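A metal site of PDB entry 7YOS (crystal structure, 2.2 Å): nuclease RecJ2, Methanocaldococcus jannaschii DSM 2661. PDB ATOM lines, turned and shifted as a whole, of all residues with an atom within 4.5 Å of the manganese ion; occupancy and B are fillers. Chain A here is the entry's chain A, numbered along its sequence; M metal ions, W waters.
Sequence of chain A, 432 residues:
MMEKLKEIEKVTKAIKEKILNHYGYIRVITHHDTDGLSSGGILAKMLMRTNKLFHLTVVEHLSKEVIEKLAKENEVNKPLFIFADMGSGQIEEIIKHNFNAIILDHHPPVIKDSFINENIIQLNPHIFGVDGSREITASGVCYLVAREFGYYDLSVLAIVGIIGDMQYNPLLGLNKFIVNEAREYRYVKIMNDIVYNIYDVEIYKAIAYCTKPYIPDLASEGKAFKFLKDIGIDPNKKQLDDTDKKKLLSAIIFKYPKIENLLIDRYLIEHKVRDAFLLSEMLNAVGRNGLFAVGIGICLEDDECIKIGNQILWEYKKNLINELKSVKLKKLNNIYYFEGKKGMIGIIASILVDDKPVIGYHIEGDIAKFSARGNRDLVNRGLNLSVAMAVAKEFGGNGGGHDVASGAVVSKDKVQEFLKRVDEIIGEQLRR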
ATOM      1  N   ASP A  35     -19.391  -6.894   0.756  1.00  0.00           N
ATOM      2  CA  ASP A  35     -19.631  -7.633  -0.479  1.00  0.00           C
ATOM      3  C   ASP A  35     -20.626  -6.923  -1.382  1.00  0.00           C
ATOM      4  O   ASP A  35     -20.513  -6.997  -2.611  1.00  0.00           O
ATOM      5  CB  ASP A  35     -20.148  -9.051  -0.156  1.00  0.00           C
ATOM      6  CG  ASP A  35     -19.984 -10.043  -1.338  1.00  0.00           C
ATOM      7  OD1 ASP A  35     -19.171  -9.803  -2.269  1.00  0.00           O
ATOM      8  OD2 ASP A  35     -20.686 -11.069  -1.347  1.00  0.00           O
ATOM      9  N   HIS A 106     -25.401 -15.137  -4.376  1.00  0.00           N
ATOM     10  CA  HIS A 106     -24.856 -16.432  -3.987  1.00  0.00           C
ATOM     11  C   HIS A 106     -25.561 -17.042  -2.786  1.00  0.00           C
ATOM     12  O   HIS A 106     -25.047 -18.013  -2.210  1.00  0.00           O
ATOM     13  CB  HIS A 106     -23.334 -16.346  -3.741  1.00  0.00           C
ATOM     14  CG  HIS A 106     -22.944 -15.539  -2.539  1.00  0.00           C
ATOM     15  ND1 HIS A 106     -21.957 -15.933  -1.666  1.00  0.00           N
ATOM     16  CD2 HIS A 106     -23.364 -14.334  -2.092  1.00  0.00           C
ATOM     17  CE1 HIS A 106     -21.817 -15.023  -0.718  1.00  0.00           C
ATOM     18  NE2 HIS A 106     -22.654 -14.041  -0.959  1.00  0.00           N
ATOM     19  N   ALA A 138     -20.961 -12.428  -3.782  1.00  0.00           N
ATOM     20  CA  ALA A 138     -21.678 -11.575  -4.731  1.00  0.00           C
ATOM     21  C   ALA A 138     -20.703 -10.759  -5.584  1.00  0.00           C
ATOM     22  O   ALA A 138     -20.909 -10.605  -6.794  1.00  0.00           O
ATOM     23  CB  ALA A 138     -22.637 -10.639  -3.996  1.00  0.00           C
ATOM     24  N   ASP A 165     -16.601 -11.353   3.099  1.00  0.00           N
ATOM     25  CA  ASP A 165     -17.451 -12.504   3.379  1.00  0.00           C
ATOM     26  C   ASP A 165     -16.684 -13.671   3.989  1.00  0.00           C
ATOM     27  O   ASP A 165     -17.232 -14.783   4.046  1.00  0.00           O
ATOM     28  CB  ASP A 165     -18.160 -12.952   2.096  1.00  0.00           C
ATOM     29  CG  ASP A 165     -19.527 -12.318   1.939  1.00  0.00           C
ATOM     30  OD1 ASP A 165     -19.834 -11.327   2.643  1.00  0.00           O
ATOM     31  OD2 ASP A 165     -20.321 -12.823   1.124  1.00  0.00           O
HETATM   32 MN    MN M   1     -22.249 -11.980   0.361  1.00  0.00          MN
HETATM   33  O   HOH W   1     -23.773 -13.384   1.853  1.00  0.00           O
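The manganese ion is bound by OD2 of Asp 165 (2.2 Å).
A ring nitrogen (NE2) of His 106 is bound to the manganese ion, 2.5 Å away.
OD2 of Asp 35 binds the manganese ion, 2.5 Å away.
The manganese ion is bound by water W1 (2.6 Å).
The manganese ion has four donor atoms within binding distance.
OD2 of Asp 35 lies close to N of Ala 138, 2.8 Å away.
Three residues have an atom within 4 Å of the manganese ion: Asp 35, His 106 and Asp 165.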
